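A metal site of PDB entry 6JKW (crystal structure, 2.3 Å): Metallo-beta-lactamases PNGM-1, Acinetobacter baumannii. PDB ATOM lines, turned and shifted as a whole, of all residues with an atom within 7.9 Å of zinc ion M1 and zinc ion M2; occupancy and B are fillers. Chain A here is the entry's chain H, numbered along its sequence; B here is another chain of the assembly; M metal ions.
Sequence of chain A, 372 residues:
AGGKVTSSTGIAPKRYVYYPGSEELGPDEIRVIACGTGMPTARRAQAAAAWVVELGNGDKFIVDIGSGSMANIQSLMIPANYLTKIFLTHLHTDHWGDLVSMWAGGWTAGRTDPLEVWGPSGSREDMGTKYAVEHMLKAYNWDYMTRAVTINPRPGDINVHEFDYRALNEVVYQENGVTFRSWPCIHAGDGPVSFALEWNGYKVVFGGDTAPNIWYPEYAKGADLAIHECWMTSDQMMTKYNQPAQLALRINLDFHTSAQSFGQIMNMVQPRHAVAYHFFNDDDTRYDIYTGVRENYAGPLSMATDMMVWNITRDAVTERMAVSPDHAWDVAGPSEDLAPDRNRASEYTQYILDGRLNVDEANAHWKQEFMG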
ATOM      1  N   GLY A  38      18.669  10.250 -38.041  1.00  0.00           N
ATOM      2  CA  GLY A  38      19.197   8.976 -37.597  1.00  0.00           C
ATOM      3  C   GLY A  38      19.727   8.901 -36.155  1.00  0.00           C
ATOM      4  O   GLY A  38      19.190   9.570 -35.250  1.00  0.00           O
ATOM      5  N   MET A  39      20.765   8.061 -35.983  1.00  0.00           N
ATOM      6  CA  MET A  39      21.350   7.640 -34.703  1.00  0.00           C
ATOM      7  C   MET A  39      22.823   7.955 -34.709  1.00  0.00           C
ATOM      8  O   MET A  39      23.372   8.328 -35.756  1.00  0.00           O
ATOM      9  CB  MET A  39      21.220   6.126 -34.633  1.00  0.00           C
ATOM     10  CG  MET A  39      19.781   5.616 -34.579  1.00  0.00           C
ATOM     11  SD  MET A  39      19.219   5.477 -32.703  1.00  0.00           S
ATOM     12  CE  MET A  39      19.192   3.501 -32.594  1.00  0.00           C
ATOM     13  N   PRO A  40      23.507   7.788 -33.554  1.00  0.00           N
ATOM     14  CA  PRO A  40      24.987   7.908 -33.601  1.00  0.00           C
ATOM     15  C   PRO A  40      25.650   6.812 -34.459  1.00  0.00           C
ATOM     16  O   PRO A  40      26.785   6.998 -34.883  1.00  0.00           O
ATOM     17  CB  PRO A  40      25.405   7.778 -32.129  1.00  0.00           C
ATOM     18  CG  PRO A  40      24.252   7.067 -31.459  1.00  0.00           C
ATOM     19  CD  PRO A  40      23.014   7.538 -32.183  1.00  0.00           C
ATOM     20  N   ALA A  48      22.803  11.646 -39.529  1.00  0.00           N
ATOM     21  CA  ALA A  48      22.436  11.978 -38.120  1.00  0.00           C
ATOM     22  C   ALA A  48      21.644  13.310 -38.084  1.00  0.00           C
ATOM     23  O   ALA A  48      21.709  14.069 -39.053  1.00  0.00           O
ATOM     24  CB  ALA A  48      23.659  12.059 -37.218  1.00  0.00           C
ATOM     25  N   ALA A  49      20.940  13.583 -36.994  1.00  0.00           N
ATOM     26  CA  ALA A  49      19.969  14.725 -36.854  1.00  0.00           C
ATOM     27  C   ALA A  49      20.401  16.034 -37.426  1.00  0.00           C
ATOM     28  O   ALA A  49      21.351  16.562 -36.932  1.00  0.00           O
ATOM     29  CB  ALA A  49      19.678  14.960 -35.378  1.00  0.00           C
ATOM     30  N   ASP A  64      20.854  21.809 -35.832  1.00  0.00           N
ATOM     31  CA  ASP A  64      21.559  20.514 -35.675  1.00  0.00           C
ATOM     32  C   ASP A  64      22.193  20.162 -37.017  1.00  0.00           C
ATOM     33  O   ASP A  64      21.673  20.533 -38.103  1.00  0.00           O
ATOM     34  CB  ASP A  64      20.714  19.398 -34.998  1.00  0.00           C
ATOM     35  CG  ASP A  64      20.690  19.547 -33.502  1.00  0.00           C
ATOM     36  OD1 ASP A  64      21.326  20.521 -33.083  1.00  0.00           O
ATOM     37  OD2 ASP A  64      20.143  18.742 -32.723  1.00  0.00           O
ATOM     38  N   THR A  89      21.269  21.966 -30.489  1.00  0.00           N
ATOM     39  CA  THR A  89      20.533  21.530 -29.344  1.00  0.00           C
ATOM     40  C   THR A  89      21.433  20.903 -28.306  1.00  0.00           C
ATOM     41  O   THR A  89      21.103  20.922 -27.123  1.00  0.00           O
ATOM     42  CB  THR A  89      19.455  20.499 -29.725  1.00  0.00           C
ATOM     43  OG1 THR A  89      20.066  19.302 -30.242  1.00  0.00           O
ATOM     44  CG2 THR A  89      18.464  21.103 -30.777  1.00  0.00           C
ATOM     45  N   HIS A  90      22.520  20.265 -28.741  1.00  0.00           N
ATOM     46  CA  HIS A  90      23.477  19.629 -27.826  1.00  0.00           C
ATOM     47  C   HIS A  90      24.741  19.102 -28.508  1.00  0.00           C
ATOM     48  O   HIS A  90      24.876  19.146 -29.730  1.00  0.00           O
ATOM     49  CB  HIS A  90      22.830  18.559 -26.963  1.00  0.00           C
ATOM     50  CG  HIS A  90      22.468  17.269 -27.671  1.00  0.00           C
ATOM     51  ND1 HIS A  90      21.450  17.180 -28.598  1.00  0.00           N
ATOM     52  CD2 HIS A  90      22.902  15.999 -27.465  1.00  0.00           C
ATOM     53  CE1 HIS A  90      21.287  15.927 -28.935  1.00  0.00           C
ATOM     54  NE2 HIS A  90      22.172  15.185 -28.291  1.00  0.00           N
ATOM     55  N   LEU A  91      25.654  18.574 -27.710  1.00  0.00           N
ATOM     56  CA  LEU A  91      27.040  18.462 -28.152  1.00  0.00           C
ATOM     57  C   LEU A  91      27.456  17.068 -28.580  1.00  0.00           C
ATOM     58  O   LEU A  91      28.591  16.863 -28.993  1.00  0.00           O
ATOM     59  CB  LEU A  91      27.990  19.019 -27.075  1.00  0.00           C
ATOM     60  CG  LEU A  91      27.899  20.559 -27.014  1.00  0.00           C
ATOM     61  CD1 LEU A  91      28.775  21.058 -25.862  1.00  0.00           C
ATOM     62  CD2 LEU A  91      28.233  21.283 -28.324  1.00  0.00           C
ATOM     63  N   HIS A  92      26.510  16.122 -28.509  1.00  0.00           N
ATOM     64  CA  HIS A  92      26.685  14.830 -29.118  1.00  0.00           C
ATOM     65  C   HIS A  92      27.137  14.911 -30.593  1.00  0.00           C
ATOM     66  O   HIS A  92      26.758  15.795 -31.334  1.00  0.00           O
ATOM     67  CB  HIS A  92      25.470  13.978 -28.976  1.00  0.00           C
ATOM     68  CG  HIS A  92      25.418  13.140 -27.742  1.00  0.00           C
ATOM     69  ND1 HIS A  92      24.219  12.797 -27.164  1.00  0.00           N
ATOM     70  CD2 HIS A  92      26.368  12.520 -27.015  1.00  0.00           C
ATOM     71  CE1 HIS A  92      24.424  11.978 -26.157  1.00  0.00           C
ATOM     72  NE2 HIS A  92      25.721  11.788 -26.037  1.00  0.00           N
ATOM     73  N   THR A  93      28.028  13.986 -30.976  1.00  0.00           N
ATOM     74  CA  THR A  93      28.641  13.999 -32.350  1.00  0.00           C
ATOM     75  C   THR A  93      27.546  13.933 -33.404  1.00  0.00           C
ATOM     76  O   THR A  93      27.630  14.605 -34.432  1.00  0.00           O
ATOM     77  CB  THR A  93      29.619  12.799 -32.556  1.00  0.00           C
ATOM     78  OG1 THR A  93      28.880  11.580 -32.471  1.00  0.00           O
ATOM     79  CG2 THR A  93      30.710  12.795 -31.446  1.00  0.00           C
ATOM     80  N   ASP A  94      26.498  13.195 -33.135  1.00  0.00           N
ATOM     81  CA  ASP A  94      25.418  13.114 -34.087  1.00  0.00           C
ATOM     82  C   ASP A  94      24.534  14.399 -34.186  1.00  0.00           C
ATOM     83  O   ASP A  94      23.576  14.413 -34.958  1.00  0.00           O
ATOM     84  CB  ASP A  94      24.565  11.833 -33.882  1.00  0.00           C
ATOM     85  CG  ASP A  94      23.987  11.684 -32.480  1.00  0.00           C
ATOM     86  OD1 ASP A  94      22.936  10.991 -32.327  1.00  0.00           O
ATOM     87  OD2 ASP A  94      24.594  12.192 -31.515  1.00  0.00           O
ATOM     88  N   HIS A  95      24.868  15.488 -33.457  1.00  0.00           N
ATOM     89  CA  HIS A  95      24.167  16.779 -33.651  1.00  0.00           C
ATOM     90  C   HIS A  95      25.001  17.952 -34.081  1.00  0.00           C
ATOM     91  O   HIS A  95      24.405  18.998 -34.370  1.00  0.00           O
ATOM     92  CB  HIS A  95      23.375  17.152 -32.428  1.00  0.00           C
ATOM     93  CG  HIS A  95      22.360  16.124 -32.083  1.00  0.00           C
ATOM     94  ND1 HIS A  95      21.023  16.259 -32.400  1.00  0.00           N
ATOM     95  CD2 HIS A  95      22.499  14.914 -31.503  1.00  0.00           C
ATOM     96  CE1 HIS A  95      20.374  15.178 -31.988  1.00  0.00           C
ATOM     97  NE2 HIS A  95      21.240  14.338 -31.448  1.00  0.00           N
ATOM     98  N   HIS A 187      19.124  14.646 -21.065  1.00  0.00           N
ATOM     99  CA  HIS A 187      19.904  13.786 -21.982  1.00  0.00           C
ATOM    100  C   HIS A 187      21.400  13.675 -21.567  1.00  0.00           C
ATOM    101  O   HIS A 187      22.183  14.561 -21.821  1.00  0.00           O
ATOM    102  CB  HIS A 187      19.782  14.367 -23.418  1.00  0.00           C
ATOM    103  CG  HIS A 187      20.344  13.501 -24.495  1.00  0.00           C
ATOM    104  ND1 HIS A 187      20.085  12.152 -24.570  1.00  0.00           N
ATOM    105  CD2 HIS A 187      21.139  13.796 -25.552  1.00  0.00           C
ATOM    106  CE1 HIS A 187      20.697  11.647 -25.630  1.00  0.00           C
ATOM    107  NE2 HIS A 187      21.331  12.618 -26.252  1.00  0.00           N
ATOM    108  N   ALA A 188      21.764  12.572 -20.929  1.00  0.00           N
ATOM    109  CA  ALA A 188      23.188  12.197 -20.695  1.00  0.00           C
ATOM    110  C   ALA A 188      23.926  13.034 -19.637  1.00  0.00           C
ATOM    111  O   ALA A 188      24.765  12.518 -18.915  1.00  0.00           O
ATOM    112  CB  ALA A 188      23.970  12.130 -21.999  1.00  0.00           C
ATOM    113  N   PRO A 192      22.091  19.902 -22.710  1.00  0.00           N
ATOM    114  CA  PRO A 192      21.240  19.754 -23.882  1.00  0.00           C
ATOM    115  C   PRO A 192      19.835  20.371 -23.719  1.00  0.00           C
ATOM    116  O   PRO A 192      19.211  20.208 -22.660  1.00  0.00           O
ATOM    117  CB  PRO A 192      21.095  18.244 -24.035  1.00  0.00           C
ATOM    118  CG  PRO A 192      21.981  17.621 -23.047  1.00  0.00           C
ATOM    119  CD  PRO A 192      22.320  18.628 -22.020  1.00  0.00           C
ATOM    120  N   GLY A 208      15.408  18.403 -30.080  1.00  0.00           N
ATOM    121  CA  GLY A 208      16.712  17.730 -29.875  1.00  0.00           C
ATOM    122  C   GLY A 208      16.442  16.346 -29.291  1.00  0.00           C
ATOM    123  O   GLY A 208      15.584  15.616 -29.807  1.00  0.00           O
ATOM    124  N   ASP A 209      17.168  15.976 -28.241  1.00  0.00           N
ATOM    125  CA  ASP A 209      16.998  14.679 -27.563  1.00  0.00           C
ATOM    126  C   ASP A 209      16.668  14.907 -26.095  1.00  0.00           C
ATOM    127  O   ASP A 209      17.205  15.839 -25.461  1.00  0.00           O
ATOM    128  CB  ASP A 209      18.313  13.871 -27.521  1.00  0.00           C
ATOM    129  CG  ASP A 209      18.840  13.454 -28.881  1.00  0.00           C
ATOM    130  OD1 ASP A 209      18.423  14.008 -29.926  1.00  0.00           O
ATOM    131  OD2 ASP A 209      19.737  12.561 -28.887  1.00  0.00           O
ATOM    132  N   THR A 210      15.887  14.001 -25.526  1.00  0.00           N
ATOM    133  CA  THR A 210      15.549  14.087 -24.133  1.00  0.00           C
ATOM    134  C   THR A 210      14.837  12.896 -23.706  1.00  0.00           C
ATOM    135  O   THR A 210      14.154  12.288 -24.521  1.00  0.00           O
ATOM    136  CB  THR A 210      14.548  15.218 -23.795  1.00  0.00           C
ATOM    137  OG1 THR A 210      14.229  15.146 -22.389  1.00  0.00           O
ATOM    138  CG2 THR A 210      13.251  15.108 -24.644  1.00  0.00           C
ATOM    139  N   GLU A 229      12.173  13.611 -29.956  1.00  0.00           N
ATOM    140  CA  GLU A 229      12.762  12.259 -29.995  1.00  0.00           C
ATOM    141  C   GLU A 229      11.714  11.172 -29.712  1.00  0.00           C
ATOM    142  O   GLU A 229      10.832  11.370 -28.886  1.00  0.00           O
ATOM    143  CB  GLU A 229      13.946  12.118 -28.992  1.00  0.00           C
ATOM    144  CG  GLU A 229      13.904  10.835 -28.113  1.00  0.00           C
ATOM    145  CD  GLU A 229      15.066  10.637 -27.109  1.00  0.00           C
ATOM    146  OE1 GLU A 229      16.058  11.412 -27.079  1.00  0.00           O
ATOM    147  OE2 GLU A 229      14.920   9.671 -26.309  1.00  0.00           O
ATOM    148  N   TRP A 231      11.954   6.766 -29.505  1.00  0.00           N
ATOM    149  CA  TRP A 231      12.933   5.709 -29.551  1.00  0.00           C
ATOM    150  C   TRP A 231      12.361   4.394 -30.032  1.00  0.00           C
ATOM    151  O   TRP A 231      11.155   4.154 -29.910  1.00  0.00           O
ATOM    152  CB  TRP A 231      13.520   5.511 -28.140  1.00  0.00           C
ATOM    153  CG  TRP A 231      14.904   4.995 -28.086  1.00  0.00           C
ATOM    154  CD1 TRP A 231      15.292   3.750 -27.693  1.00  0.00           C
ATOM    155  CD2 TRP A 231      16.087   5.700 -28.428  1.00  0.00           C
ATOM    156  NE1 TRP A 231      16.658   3.650 -27.781  1.00  0.00           N
ATOM    157  CE2 TRP A 231      17.175   4.830 -28.230  1.00  0.00           C
ATOM    158  CE3 TRP A 231      16.335   7.001 -28.881  1.00  0.00           C
ATOM    159  CZ2 TRP A 231      18.486   5.202 -28.459  1.00  0.00           C
ATOM    160  CZ3 TRP A 231      17.620   7.368 -29.133  1.00  0.00           C
ATOM    161  CH2 TRP A 231      18.695   6.482 -28.921  1.00  0.00           C
ATOM    162  N   HIS A 256      15.472   7.174 -22.516  1.00  0.00           N
ATOM    163  CA  HIS A 256      14.898   7.821 -23.697  1.00  0.00           C
ATOM    164  C   HIS A 256      13.369   7.923 -23.602  1.00  0.00           C
ATOM    165  O   HIS A 256      12.732   7.303 -22.761  1.00  0.00           O
ATOM    166  CB  HIS A 256      15.261   7.038 -24.972  1.00  0.00           C
ATOM    167  CG  HIS A 256      16.732   6.830 -25.181  1.00  0.00           C
ATOM    168  ND1 HIS A 256      17.518   7.732 -25.865  1.00  0.00           N
ATOM    169  CD2 HIS A 256      17.553   5.819 -24.816  1.00  0.00           C
ATOM    170  CE1 HIS A 256      18.768   7.304 -25.889  1.00  0.00           C
ATOM    171  NE2 HIS A 256      18.815   6.144 -25.263  1.00  0.00           N
ATOM    172  N   TYR A 277      11.113  11.519 -34.369  1.00  0.00           N
ATOM    173  CA  TYR A 277      12.407  11.192 -34.977  1.00  0.00           C
ATOM    174  C   TYR A 277      13.384  10.561 -34.031  1.00  0.00           C
ATOM    175  O   TYR A 277      13.126  10.446 -32.841  1.00  0.00           O
ATOM    176  CB  TYR A 277      13.057  12.415 -35.636  1.00  0.00           C
ATOM    177  CG  TYR A 277      14.020  13.186 -34.737  1.00  0.00           C
ATOM    178  CD1 TYR A 277      13.596  13.775 -33.533  1.00  0.00           C
ATOM    179  CD2 TYR A 277      15.341  13.343 -35.099  1.00  0.00           C
ATOM    180  CE1 TYR A 277      14.475  14.474 -32.726  1.00  0.00           C
ATOM    181  CE2 TYR A 277      16.227  14.042 -34.299  1.00  0.00           C
ATOM    182  CZ  TYR A 277      15.817  14.619 -33.112  1.00  0.00           C
ATOM    183  OH  TYR A 277      16.752  15.323 -32.349  1.00  0.00           O
ATOM    184  N   HIS A 278      14.520  10.157 -34.610  1.00  0.00           N
ATOM    185  CA  HIS A 278      15.674   9.622 -33.912  1.00  0.00           C
ATOM    186  C   HIS A 278      15.626   8.133 -33.783  1.00  0.00           C
ATOM    187  O   HIS A 278      16.119   7.581 -32.818  1.00  0.00           O
ATOM    188  CB  HIS A 278      15.844  10.226 -32.532  1.00  0.00           C
ATOM    189  CG  HIS A 278      17.271  10.547 -32.208  1.00  0.00           C
ATOM    190  ND1 HIS A 278      18.118   9.662 -31.571  1.00  0.00           N
ATOM    191  CD2 HIS A 278      17.977  11.669 -32.423  1.00  0.00           C
ATOM    192  CE1 HIS A 278      19.292  10.244 -31.394  1.00  0.00           C
ATOM    193  NE2 HIS A 278      19.220  11.470 -31.889  1.00  0.00           N
ATOM    194  N   TRP B 142      32.147  17.192 -24.072  1.00  0.00           N
ATOM    195  CA  TRP B 142      30.798  16.961 -23.505  1.00  0.00           C
ATOM    196  C   TRP B 142      30.358  15.563 -23.896  1.00  0.00           C
ATOM    197  O   TRP B 142      29.863  14.804 -23.055  1.00  0.00           O
ATOM    198  CB  TRP B 142      29.777  17.969 -23.974  1.00  0.00           C
ATOM    199  CG  TRP B 142      28.440  17.770 -23.288  1.00  0.00           C
ATOM    200  CD1 TRP B 142      28.009  18.378 -22.140  1.00  0.00           C
ATOM    201  CD2 TRP B 142      27.378  16.926 -23.700  1.00  0.00           C
ATOM    202  NE1 TRP B 142      26.794  17.920 -21.800  1.00  0.00           N
ATOM    203  CE2 TRP B 142      26.348  17.061 -22.757  1.00  0.00           C
ATOM    204  CE3 TRP B 142      27.188  16.078 -24.794  1.00  0.00           C
ATOM    205  CZ2 TRP B 142      25.134  16.379 -22.859  1.00  0.00           C
ATOM    206  CZ3 TRP B 142      25.980  15.388 -24.893  1.00  0.00           C
ATOM    207  CH2 TRP B 142      24.970  15.542 -23.917  1.00  0.00           C
ATOM    208  N   ASP B 143      30.600  15.197 -25.190  1.00  0.00           N
ATOM    209  CA  ASP B 143      30.298  13.850 -25.631  1.00  0.00           C
ATOM    210  C   ASP B 143      31.101  12.827 -24.808  1.00  0.00           C
ATOM    211  O   ASP B 143      30.547  11.877 -24.235  1.00  0.00           O
ATOM    212  CB  ASP B 143      30.521  13.688 -27.156  1.00  0.00           C
ATOM    213  CG  ASP B 143      29.742  12.475 -27.736  1.00  0.00           C
ATOM    214  OD1 ASP B 143      29.788  11.394 -27.115  1.00  0.00           O
ATOM    215  OD2 ASP B 143      29.023  12.630 -28.763  1.00  0.00           O
HETATM  216 ZN    ZN M   1      21.136  12.341 -30.710  1.00  0.00          ZN
HETATM  217 ZN    ZN M   2      22.058  13.059 -27.956  1.00  0.00          ZN
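Zinc ion M1 is bound by NE2 of His 95 (2.1 Å), OD2 of Asp 209 (2.3 Å) and NE2 of His 278 (2.4 Å).
Zinc ion M1 has three donor atoms within binding distance.
Slightly farther from zinc ion M1 lies the side-chain carboxylate (OD1) of Asp 94 (2.8 Å).
NE2 of His 187 is bound to zinc ion M2 (1.9 Å).
Zinc ion M2 is bound by NE2 of His 90.
Zinc ion M2 is bound by a ring nitrogen (ND1) of His 92 (2.3 Å).
The side-chain carboxylate (OD2) of Asp 209 is bound to zinc ion M2, at 2.5 Å.
A ring nitrogen (ND1) of His 95 lies within hydrogen-bond range of the side-chain carboxylate of Asp 64, 2.7 Å away.
A ring nitrogen (ND1) of His 90 is in hydrogen-bond range of the side-chain hydroxyl (OG1) of Thr 89 (3.0 Å).
The side-chain carboxylate (OD1) of Asp 209 is in hydrogen-bond range of the side-chain hydroxyl (OH) of Tyr 277 (3.2 Å).
O of Asp 94 is in hydrogen-bond range of N of Ala 49, at 3.4 Å.
Five residues have an atom within 4 Å of zinc ion M1: His 90, Asp 94, His 95, Asp 209 and His 278.
Five residues have an atom within 4 Å of zinc ion M2: His 90, His 92, His 95, His 187 and Asp 209.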
